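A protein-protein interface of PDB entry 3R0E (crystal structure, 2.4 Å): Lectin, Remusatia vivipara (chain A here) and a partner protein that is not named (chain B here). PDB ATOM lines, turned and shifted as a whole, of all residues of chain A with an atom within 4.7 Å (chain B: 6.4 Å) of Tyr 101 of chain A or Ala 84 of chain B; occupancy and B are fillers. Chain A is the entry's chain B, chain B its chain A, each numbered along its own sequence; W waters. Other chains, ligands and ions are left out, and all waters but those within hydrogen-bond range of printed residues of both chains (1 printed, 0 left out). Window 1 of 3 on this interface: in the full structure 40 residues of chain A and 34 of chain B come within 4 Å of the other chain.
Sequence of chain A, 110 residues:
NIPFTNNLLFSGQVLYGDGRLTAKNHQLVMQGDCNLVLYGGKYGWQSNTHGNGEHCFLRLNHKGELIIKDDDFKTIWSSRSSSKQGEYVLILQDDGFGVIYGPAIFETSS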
ATOM      1  N   GLU A  87      28.372 -17.413  23.335  1.00  0.00           N
ATOM      2  CA  GLU A  87      28.590 -16.274  22.462  1.00  0.00           C
ATOM      3  C   GLU A  87      27.551 -16.239  21.312  1.00  0.00           C
ATOM      4  O   GLU A  87      27.409 -17.218  20.584  1.00  0.00           O
ATOM      5  CB  GLU A  87      30.025 -16.313  21.939  1.00  0.00           C
ATOM      6  CG  GLU A  87      30.445 -15.085  21.122  1.00  0.00           C
ATOM      7  CD  GLU A  87      31.880 -15.187  20.578  1.00  0.00           C
ATOM      8  OE1 GLU A  87      32.332 -14.210  19.947  1.00  0.00           O
ATOM      9  OE2 GLU A  87      32.553 -16.236  20.784  1.00  0.00           O
ATOM     10  N   TYR A  88      26.830 -15.124  21.164  1.00  0.00           N
ATOM     11  CA  TYR A  88      25.846 -14.974  20.088  1.00  0.00           C
ATOM     12  C   TYR A  88      26.141 -13.783  19.181  1.00  0.00           C
ATOM     13  O   TYR A  88      26.800 -12.826  19.591  1.00  0.00           O
ATOM     14  CB  TYR A  88      24.426 -14.856  20.654  1.00  0.00           C
ATOM     15  CG  TYR A  88      23.900 -16.154  21.223  1.00  0.00           C
ATOM     16  CD1 TYR A  88      24.341 -16.630  22.467  1.00  0.00           C
ATOM     17  CD2 TYR A  88      22.963 -16.912  20.522  1.00  0.00           C
ATOM     18  CE1 TYR A  88      23.879 -17.808  22.986  1.00  0.00           C
ATOM     19  CE2 TYR A  88      22.477 -18.103  21.048  1.00  0.00           C
ATOM     20  CZ  TYR A  88      22.944 -18.548  22.280  1.00  0.00           C
ATOM     21  OH  TYR A  88      22.464 -19.729  22.804  1.00  0.00           O
ATOM     22  N   VAL A  89      25.651 -13.848  17.949  1.00  0.00           N
ATOM     23  CA  VAL A  89      25.785 -12.746  17.005  1.00  0.00           C
ATOM     24  C   VAL A  89      24.447 -12.492  16.312  1.00  0.00           C
ATOM     25  O   VAL A  89      23.747 -13.440  15.944  1.00  0.00           O
ATOM     26  CB  VAL A  89      26.919 -13.004  15.963  1.00  0.00           C
ATOM     27  CG1 VAL A  89      26.630 -14.220  15.093  1.00  0.00           C
ATOM     28  CG2 VAL A  89      27.186 -11.759  15.103  1.00  0.00           C
ATOM     29  N   ILE A  91      23.222 -10.944  12.890  1.00  0.00           N
ATOM     30  CA  ILE A  91      23.725 -10.506  11.593  1.00  0.00           C
ATOM     31  C   ILE A  91      22.604  -9.856  10.783  1.00  0.00           C
ATOM     32  O   ILE A  91      21.553 -10.457  10.557  1.00  0.00           O
ATOM     33  CB  ILE A  91      24.371 -11.660  10.790  1.00  0.00           C
ATOM     34  CG1 ILE A  91      25.408 -12.405  11.638  1.00  0.00           C
ATOM     35  CG2 ILE A  91      25.020 -11.136   9.493  1.00  0.00           C
ATOM     36  CD1 ILE A  91      25.975 -13.629  10.979  1.00  0.00           C
ATOM     37  N   GLN A  93      21.902  -9.495   7.430  1.00  0.00           N
ATOM     38  CA  GLN A  93      22.416 -10.163   6.237  1.00  0.00           C
ATOM     39  C   GLN A  93      22.110  -9.388   4.966  1.00  0.00           C
ATOM     40  O   GLN A  93      21.116  -8.649   4.894  1.00  0.00           O
ATOM     41  CB  GLN A  93      21.826 -11.571   6.138  1.00  0.00           C
ATOM     42  CG  GLN A  93      21.944 -12.391   7.432  1.00  0.00           C
ATOM     43  CD  GLN A  93      21.358 -13.786   7.320  1.00  0.00           C
ATOM     44  OE1 GLN A  93      20.525 -14.080   6.445  1.00  0.00           O
ATOM     45  NE2 GLN A  93      21.796 -14.666   8.209  1.00  0.00           N
ATOM     46  N   VAL A  99      19.234 -12.115  11.622  1.00  0.00           N
ATOM     47  CA  VAL A  99      19.209 -13.433  12.264  1.00  0.00           C
ATOM     48  C   VAL A  99      20.183 -13.527  13.455  1.00  0.00           C
ATOM     49  O   VAL A  99      21.339 -13.098  13.369  1.00  0.00           O
ATOM     50  CB  VAL A  99      19.490 -14.575  11.235  1.00  0.00           C
ATOM     51  CG1 VAL A  99      19.262 -15.927  11.864  1.00  0.00           C
ATOM     52  CG2 VAL A  99      18.600 -14.436   9.983  1.00  0.00           C
ATOM     53  N   ILE A 100      19.703 -14.076  14.566  1.00  0.00           N
ATOM     54  CA  ILE A 100      20.556 -14.316  15.729  1.00  0.00           C
ATOM     55  C   ILE A 100      21.074 -15.745  15.676  1.00  0.00           C
ATOM     56  O   ILE A 100      20.297 -16.695  15.612  1.00  0.00           O
ATOM     57  CB  ILE A 100      19.822 -14.085  17.074  1.00  0.00           C
ATOM     58  CG1 ILE A 100      19.234 -12.675  17.144  1.00  0.00           C
ATOM     59  CG2 ILE A 100      20.776 -14.325  18.266  1.00  0.00           C
ATOM     60  CD1 ILE A 100      18.391 -12.436  18.381  1.00  0.00           C
ATOM     61  N   TYR A 101      22.391 -15.896  15.701  1.00  0.00           N
ATOM     62  CA  TYR A 101      22.998 -17.201  15.642  1.00  0.00           C
ATOM     63  C   TYR A 101      23.816 -17.425  16.885  1.00  0.00           C
ATOM     64  O   TYR A 101      24.568 -16.530  17.319  1.00  0.00           O
ATOM     65  CB  TYR A 101      23.959 -17.278  14.470  1.00  0.00           C
ATOM     66  CG  TYR A 101      23.333 -17.206  13.116  1.00  0.00           C
ATOM     67  CD1 TYR A 101      22.775 -18.347  12.523  1.00  0.00           C
ATOM     68  CD2 TYR A 101      23.318 -16.012  12.405  1.00  0.00           C
ATOM     69  CE1 TYR A 101      22.219 -18.293  11.268  1.00  0.00           C
ATOM     70  CE2 TYR A 101      22.778 -15.948  11.142  1.00  0.00           C
ATOM     71  CZ  TYR A 101      22.229 -17.092  10.582  1.00  0.00           C
ATOM     72  OH  TYR A 101      21.671 -17.033   9.342  1.00  0.00           O
ATOM     73  N   GLY A 102      23.712 -18.624  17.440  1.00  0.00           N
ATOM     74  CA  GLY A 102      24.612 -19.026  18.502  1.00  0.00           C
ATOM     75  C   GLY A 102      24.079 -20.209  19.275  1.00  0.00           C
ATOM     76  O   GLY A 102      22.974 -20.669  19.014  1.00  0.00           O
ATOM     77  N   TYR B   5      30.853 -13.002   6.431  1.00  0.00           N
ATOM     78  CA  TYR B   5      30.144 -14.181   6.929  1.00  0.00           C
ATOM     79  C   TYR B   5      29.795 -15.171   5.821  1.00  0.00           C
ATOM     80  O   TYR B   5      29.585 -14.777   4.667  1.00  0.00           O
ATOM     81  CB  TYR B   5      28.875 -13.777   7.682  1.00  0.00           C
ATOM     82  CG  TYR B   5      27.782 -13.216   6.793  1.00  0.00           C
ATOM     83  CD1 TYR B   5      27.618 -11.841   6.646  1.00  0.00           C
ATOM     84  CD2 TYR B   5      26.922 -14.063   6.090  1.00  0.00           C
ATOM     85  CE1 TYR B   5      26.622 -11.313   5.826  1.00  0.00           C
ATOM     86  CE2 TYR B   5      25.918 -13.549   5.253  1.00  0.00           C
ATOM     87  CZ  TYR B   5      25.771 -12.172   5.134  1.00  0.00           C
ATOM     88  OH  TYR B   5      24.787 -11.657   4.323  1.00  0.00           O
ATOM     89  N   LEU B   6      29.738 -16.451   6.189  1.00  0.00           N
ATOM     90  CA  LEU B   6      29.249 -17.502   5.307  1.00  0.00           C
ATOM     91  C   LEU B   6      28.116 -18.233   6.004  1.00  0.00           C
ATOM     92  O   LEU B   6      28.278 -18.726   7.122  1.00  0.00           O
ATOM     93  CB  LEU B   6      30.361 -18.485   4.919  1.00  0.00           C
ATOM     94  CG  LEU B   6      29.998 -19.517   3.838  1.00  0.00           C
ATOM     95  CD1 LEU B   6      29.998 -18.906   2.436  1.00  0.00           C
ATOM     96  CD2 LEU B   6      30.926 -20.718   3.888  1.00  0.00           C
ATOM     97  N   LEU B   7      26.965 -18.285   5.352  1.00  0.00           N
ATOM     98  CA  LEU B   7      25.821 -18.998   5.900  1.00  0.00           C
ATOM     99  C   LEU B   7      25.785 -20.439   5.400  1.00  0.00           C
ATOM    100  O   LEU B   7      26.325 -20.752   4.335  1.00  0.00           O
ATOM    101  CB  LEU B   7      24.514 -18.276   5.560  1.00  0.00           C
ATOM    102  CG  LEU B   7      24.421 -16.793   5.937  1.00  0.00           C
ATOM    103  CD1 LEU B   7      23.096 -16.187   5.410  1.00  0.00           C
ATOM    104  CD2 LEU B   7      24.555 -16.594   7.428  1.00  0.00           C
ATOM    105  N   SER B   8      25.145 -21.312   6.166  1.00  0.00           N
ATOM    106  CA  SER B   8      25.002 -22.710   5.760  1.00  0.00           C
ATOM    107  C   SER B   8      24.178 -22.790   4.490  1.00  0.00           C
ATOM    108  O   SER B   8      23.074 -22.239   4.430  1.00  0.00           O
ATOM    109  CB  SER B   8      24.372 -23.545   6.870  1.00  0.00           C
ATOM    110  OG  SER B   8      23.247 -22.880   7.410  1.00  0.00           O
ATOM    111  N   LEU B  55      29.382 -24.793   4.497  1.00  0.00           N
ATOM    112  CA  LEU B  55      29.029 -24.896   5.900  1.00  0.00           C
ATOM    113  C   LEU B  55      27.761 -25.739   5.994  1.00  0.00           C
ATOM    114  O   LEU B  55      26.734 -25.381   5.415  1.00  0.00           O
ATOM    115  CB  LEU B  55      28.795 -23.495   6.493  1.00  0.00           C
ATOM    116  CG  LEU B  55      28.424 -23.346   7.969  1.00  0.00           C
ATOM    117  CD1 LEU B  55      29.444 -24.023   8.877  1.00  0.00           C
ATOM    118  CD2 LEU B  55      28.269 -21.881   8.343  1.00  0.00           C
ATOM    119  N   ASN B  82      20.177 -23.597  10.870  1.00  0.00           N
ATOM    120  CA  ASN B  82      20.933 -22.601  10.102  1.00  0.00           C
ATOM    121  C   ASN B  82      22.124 -22.065  10.893  1.00  0.00           C
ATOM    122  O   ASN B  82      22.018 -21.748  12.083  1.00  0.00           O
ATOM    123  CB  ASN B  82      20.022 -21.460   9.658  1.00  0.00           C
ATOM    124  CG  ASN B  82      18.851 -21.941   8.809  1.00  0.00           C
ATOM    125  OD1 ASN B  82      18.976 -22.871   7.999  1.00  0.00           O
ATOM    126  ND2 ASN B  82      17.701 -21.315   9.002  1.00  0.00           N
ATOM    127  N   TYR B  83      23.261 -21.986  10.222  1.00  0.00           N
ATOM    128  CA  TYR B  83      24.504 -21.609  10.881  1.00  0.00           C
ATOM    129  C   TYR B  83      25.187 -20.486  10.118  1.00  0.00           C
ATOM    130  O   TYR B  83      24.896 -20.249   8.932  1.00  0.00           O
ATOM    131  CB  TYR B  83      25.444 -22.823  11.004  1.00  0.00           C
ATOM    132  CG  TYR B  83      25.005 -23.803  12.060  1.00  0.00           C
ATOM    133  CD1 TYR B  83      23.981 -24.724  11.809  1.00  0.00           C
ATOM    134  CD2 TYR B  83      25.606 -23.809  13.312  1.00  0.00           C
ATOM    135  CE1 TYR B  83      23.568 -25.615  12.785  1.00  0.00           C
ATOM    136  CE2 TYR B  83      25.198 -24.700  14.300  1.00  0.00           C
ATOM    137  CZ  TYR B  83      24.172 -25.601  14.026  1.00  0.00           C
ATOM    138  OH  TYR B  83      23.766 -26.484  15.006  1.00  0.00           O
ATOM    139  N   ALA B  84      26.084 -19.796  10.811  1.00  0.00           N
ATOM    140  CA  ALA B  84      26.818 -18.689  10.226  1.00  0.00           C
ATOM    141  C   ALA B  84      28.267 -18.753  10.666  1.00  0.00           C
ATOM    142  O   ALA B  84      28.559 -18.900  11.858  1.00  0.00           O
ATOM    143  CB  ALA B  84      26.188 -17.358  10.636  1.00  0.00           C
ATOM    144  N   ALA B  85      29.168 -18.679   9.697  1.00  0.00           N
ATOM    145  CA  ALA B  85      30.588 -18.542   9.983  1.00  0.00           C
ATOM    146  C   ALA B  85      30.948 -17.080   9.784  1.00  0.00           C
ATOM    147  O   ALA B  85      30.662 -16.504   8.747  1.00  0.00           O
ATOM    148  CB  ALA B  85      31.431 -19.443   9.077  1.00  0.00           C
ATOM    149  N   VAL B  86      31.571 -16.494  10.794  1.00  0.00           N
ATOM    150  CA  VAL B  86      31.819 -15.075  10.841  1.00  0.00           C
ATOM    151  C   VAL B  86      33.302 -14.818  11.071  1.00  0.00           C
ATOM    152  O   VAL B  86      33.923 -15.433  11.948  1.00  0.00           O
ATOM    153  CB  VAL B  86      31.034 -14.414  12.004  1.00  0.00           C
ATOM    154  CG1 VAL B  86      31.365 -12.941  12.108  1.00  0.00           C
ATOM    155  CG2 VAL B  86      29.522 -14.602  11.851  1.00  0.00           C
ATOM    156  N   VAL B  94      34.692 -17.773  13.480  1.00  0.00           N
ATOM    157  CA  VAL B  94      33.819 -18.422  14.453  1.00  0.00           C
ATOM    158  C   VAL B  94      32.571 -18.946  13.747  1.00  0.00           C
ATOM    159  O   VAL B  94      31.967 -18.235  12.939  1.00  0.00           O
ATOM    160  CB  VAL B  94      33.376 -17.450  15.595  1.00  0.00           C
ATOM    161  CG1 VAL B  94      32.602 -18.187  16.662  1.00  0.00           C
ATOM    162  CG2 VAL B  94      34.550 -16.727  16.224  1.00  0.00           C
ATOM    163  N   VAL B  95      32.186 -20.183  14.049  1.00  0.00           N
ATOM    164  CA  VAL B  95      30.888 -20.691  13.618  1.00  0.00           C
ATOM    165  C   VAL B  95      29.869 -20.551  14.746  1.00  0.00           C
ATOM    166  O   VAL B  95      30.117 -20.984  15.873  1.00  0.00           O
ATOM    167  CB  VAL B  95      30.955 -22.153  13.125  1.00  0.00           C
ATOM    168  CG1 VAL B  95      29.589 -22.626  12.697  1.00  0.00           C
ATOM    169  CG2 VAL B  95      31.943 -22.278  11.960  1.00  0.00           C
ATOM    170  N   PHE B  96      28.732 -19.929  14.425  1.00  0.00           N
ATOM    171  CA  PHE B  96      27.642 -19.722  15.372  1.00  0.00           C
ATOM    172  C   PHE B  96      26.388 -20.461  14.907  1.00  0.00           C
ATOM    173  O   PHE B  96      26.035 -20.435  13.712  1.00  0.00           O
ATOM    174  CB  PHE B  96      27.259 -18.247  15.447  1.00  0.00           C
ATOM    175  CG  PHE B  96      28.322 -17.341  15.985  1.00  0.00           C
ATOM    176  CD1 PHE B  96      28.368 -17.037  17.348  1.00  0.00           C
ATOM    177  CD2 PHE B  96      29.224 -16.733  15.129  1.00  0.00           C
ATOM    178  CE1 PHE B  96      29.323 -16.169  17.850  1.00  0.00           C
ATOM    179  CE2 PHE B  96      30.188 -15.859  15.618  1.00  0.00           C
ATOM    180  CZ  PHE B  96      30.238 -15.577  16.990  1.00  0.00           C
ATOM    181  N   GLY B  97      25.686 -21.077  15.854  1.00  0.00           N
ATOM    182  CA  GLY B  97      24.374 -21.623  15.565  1.00  0.00           C
ATOM    183  C   GLY B  97      23.880 -22.704  16.502  1.00  0.00           C
ATOM    184  O   GLY B  97      24.602 -23.124  17.412  1.00  0.00           O
ATOM    185  N   PRO B  98      22.644 -23.186  16.270  1.00  0.00           N
ATOM    186  CA  PRO B  98      21.800 -22.856  15.124  1.00  0.00           C
ATOM    187  C   PRO B  98      21.103 -21.503  15.319  1.00  0.00           C
ATOM    188  O   PRO B  98      21.205 -20.914  16.390  1.00  0.00           O
ATOM    189  CB  PRO B  98      20.757 -23.975  15.160  1.00  0.00           C
ATOM    190  CG  PRO B  98      20.526 -24.168  16.637  1.00  0.00           C
ATOM    191  CD  PRO B  98      21.900 -23.982  17.273  1.00  0.00           C
ATOM    192  N   SER B  99      20.389 -21.020  14.308  1.00  0.00           N
ATOM    193  CA  SER B  99      19.630 -19.786  14.480  1.00  0.00           C
ATOM    194  C   SER B  99      18.572 -19.905  15.573  1.00  0.00           C
ATOM    195  O   SER B  99      17.897 -20.930  15.718  1.00  0.00           O
ATOM    196  CB  SER B  99      18.988 -19.329  13.171  1.00  0.00           C
ATOM    197  OG  SER B  99      18.017 -20.256  12.739  1.00  0.00           O
ATOM    198  N   VAL B 100      18.420 -18.820  16.319  1.00  0.00           N
ATOM    199  CA  VAL B 100      17.546 -18.780  17.468  1.00  0.00           C
ATOM    200  C   VAL B 100      16.328 -17.865  17.210  1.00  0.00           C
ATOM    201  O   VAL B 100      15.264 -18.039  17.816  1.00  0.00           O
ATOM    202  CB  VAL B 100      18.382 -18.331  18.685  1.00  0.00           C
ATOM    203  CG1 VAL B 100      17.535 -17.749  19.752  1.00  0.00           C
ATOM    204  CG2 VAL B 100      19.220 -19.510  19.220  1.00  0.00           C
ATOM    205  N   PHE B 101      16.488 -16.922  16.280  1.00  0.00           N
ATOM    206  CA  PHE B 101      15.510 -15.857  16.028  1.00  0.00           C
ATOM    207  C   PHE B 101      15.789 -15.221  14.678  1.00  0.00           C
ATOM    208  O   PHE B 101      16.945 -15.099  14.259  1.00  0.00           O
ATOM    209  CB  PHE B 101      15.587 -14.782  17.132  1.00  0.00           C
ATOM    210  CG  PHE B 101      14.573 -13.673  16.996  1.00  0.00           C
ATOM    211  CD1 PHE B 101      13.214 -13.908  17.234  1.00  0.00           C
ATOM    212  CD2 PHE B 101      14.980 -12.380  16.667  1.00  0.00           C
ATOM    213  CE1 PHE B 101      12.268 -12.877  17.124  1.00  0.00           C
ATOM    214  CE2 PHE B 101      14.046 -11.339  16.554  1.00  0.00           C
ATOM    215  CZ  PHE B 101      12.689 -11.589  16.785  1.00  0.00           C
HETATM  216  O   HOH W   1      22.283 -19.498   8.183  1.00  0.00           O
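Water W1 lies within hydrogen-bond range of OH of Tyr 101 of chain A (2.8 Å) and O of Tyr 83 of chain B (2.8 Å).
Printed residues of chain A that touch a printed residue of chain B: Glu 87, Tyr 88, Val 89, Ile 91, Gln 93, Val 99, Ile 100, Tyr 101 and Gly 102. Hydrophobic or aromatic side chains of chain A within 4 Å of the printed part of chain B: Tyr 88, Val 89, Ile 91, Val 99, Ile 100 and Tyr 101. Hydrophobic or aromatic side chains of chain B that line the printed part of chain A: Tyr 5, Leu 7, Ala 84, Val 86, Phe 96, Pro 98, Val 100 and Phe 101.
The side-chain hydroxyl (OG) of Ser 8 of chain B is in hydrogen-bond range of the backbone NH (N) of Tyr 83 of chain B. The backbone NH (N) of Phe 96 of chain B lies within hydrogen-bond range of the backbone carbonyl oxygen (O) of Ala 84 of chain B (2.8 Å). The backbone NH (N) of Val 86 of chain B sits at hydrogen-bond distance from the backbone carbonyl oxygen (O) of Val 94 of chain B (2.8 Å). The backbone carbonyl oxygen of Val 89 of chain A sits at hydrogen-bond distance from the backbone NH of Tyr 101 of chain A, 2.8 Å away. The backbone NH of Ile 91 of chain A is in hydrogen-bond range of the backbone carbonyl oxygen of Val 99 of chain A, 2.9 Å away. NE2 of Gln 93 of chain A lies within hydrogen-bond range of OH of Tyr 101 of chain A.
N of Val 100 of chain B sits at hydrogen-bond distance from O of Ile 100 of chain A (2.9 Å). The backbone carbonyl oxygen of Phe 101 of chain B sits at hydrogen-bond distance from the backbone NH of Ile 100 of chain A, at 3.0 Å. O of Gly 97 of chain B lies close to O of Gly 102 of chain A. The backbone carbonyl oxygen (O) of Pro 98 of chain B sits close to the backbone carbonyl oxygen (O) of Gly 102 of chain A, at 3.2 Å.
Ala 84 of chain B touches just these residues of chain A: Ile 91 and Tyr 101. Of the printed residues of chain A, Val 100 of chain B touches Tyr 88, Ile 100 and Gly 102. Of the printed residues of chain A, Tyr 83 of chain B touches Tyr 101 (3.9 Å). Of the printed residues of chain A, Val 86 of chain B touches Ile 91. Printed residues of chain B within 4 Å of Glu 87 of chain A: Phe 96. Ala 85 of chain B touches none of the printed residues of chain A. Val 94 of chain B touches none of the printed residues of chain A. The nearest residue of chain B that does not touch Tyr 101 of chain A is Pro 98 of chain B (4.2 Å). The nearest printed residue of chain A that does not touch Ala 84 of chain B is Val 89 of chain A (5.5 Å).
Among the printed residues, pairs that only touch across the chains: Ile 100 of chain A with Ser 99 of chain B (3.4 Å), Glu 87 of chain A with Phe 96 of chain B (3.4 Å), Gln 93 of chain A with Tyr 5 of chain B (3.4 Å), Val 99 of chain A with Phe 101 of chain B (3.4 Å), Gln 93 of chain A with Leu 7 of chain B (3.4 Å), Tyr 101 of chain A with Leu 7 of chain B (3.5 Å), Tyr 101 of chain A with Asn 82 of chain B (3.5 Å), Tyr 101 of chain A with Phe 96 of chain B (3.6 Å), Val 89 of chain A with Phe 96 of chain B (3.6 Å), Tyr 101 of chain A with Ala 84 of chain B (3.6 Å), Val 99 of chain A with Ser 99 of chain B (3.7 Å), Ile 91 of chain A with Ala 84 of chain B (3.8 Å), Ile 91 of chain A with Val 86 of chain B (3.8 Å), Tyr 101 of chain A with Tyr 83 of chain B (3.9 Å), Tyr 101 of chain A with Ser 99 of chain B (3.9 Å), Ile 91 of chain A with Tyr 5 of chain B (3.9 Å), Gly 102 of chain A with Val 100 of chain B (3.9 Å) and Tyr 88 of chain A with Val 100 of chain B (3.99 Å).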
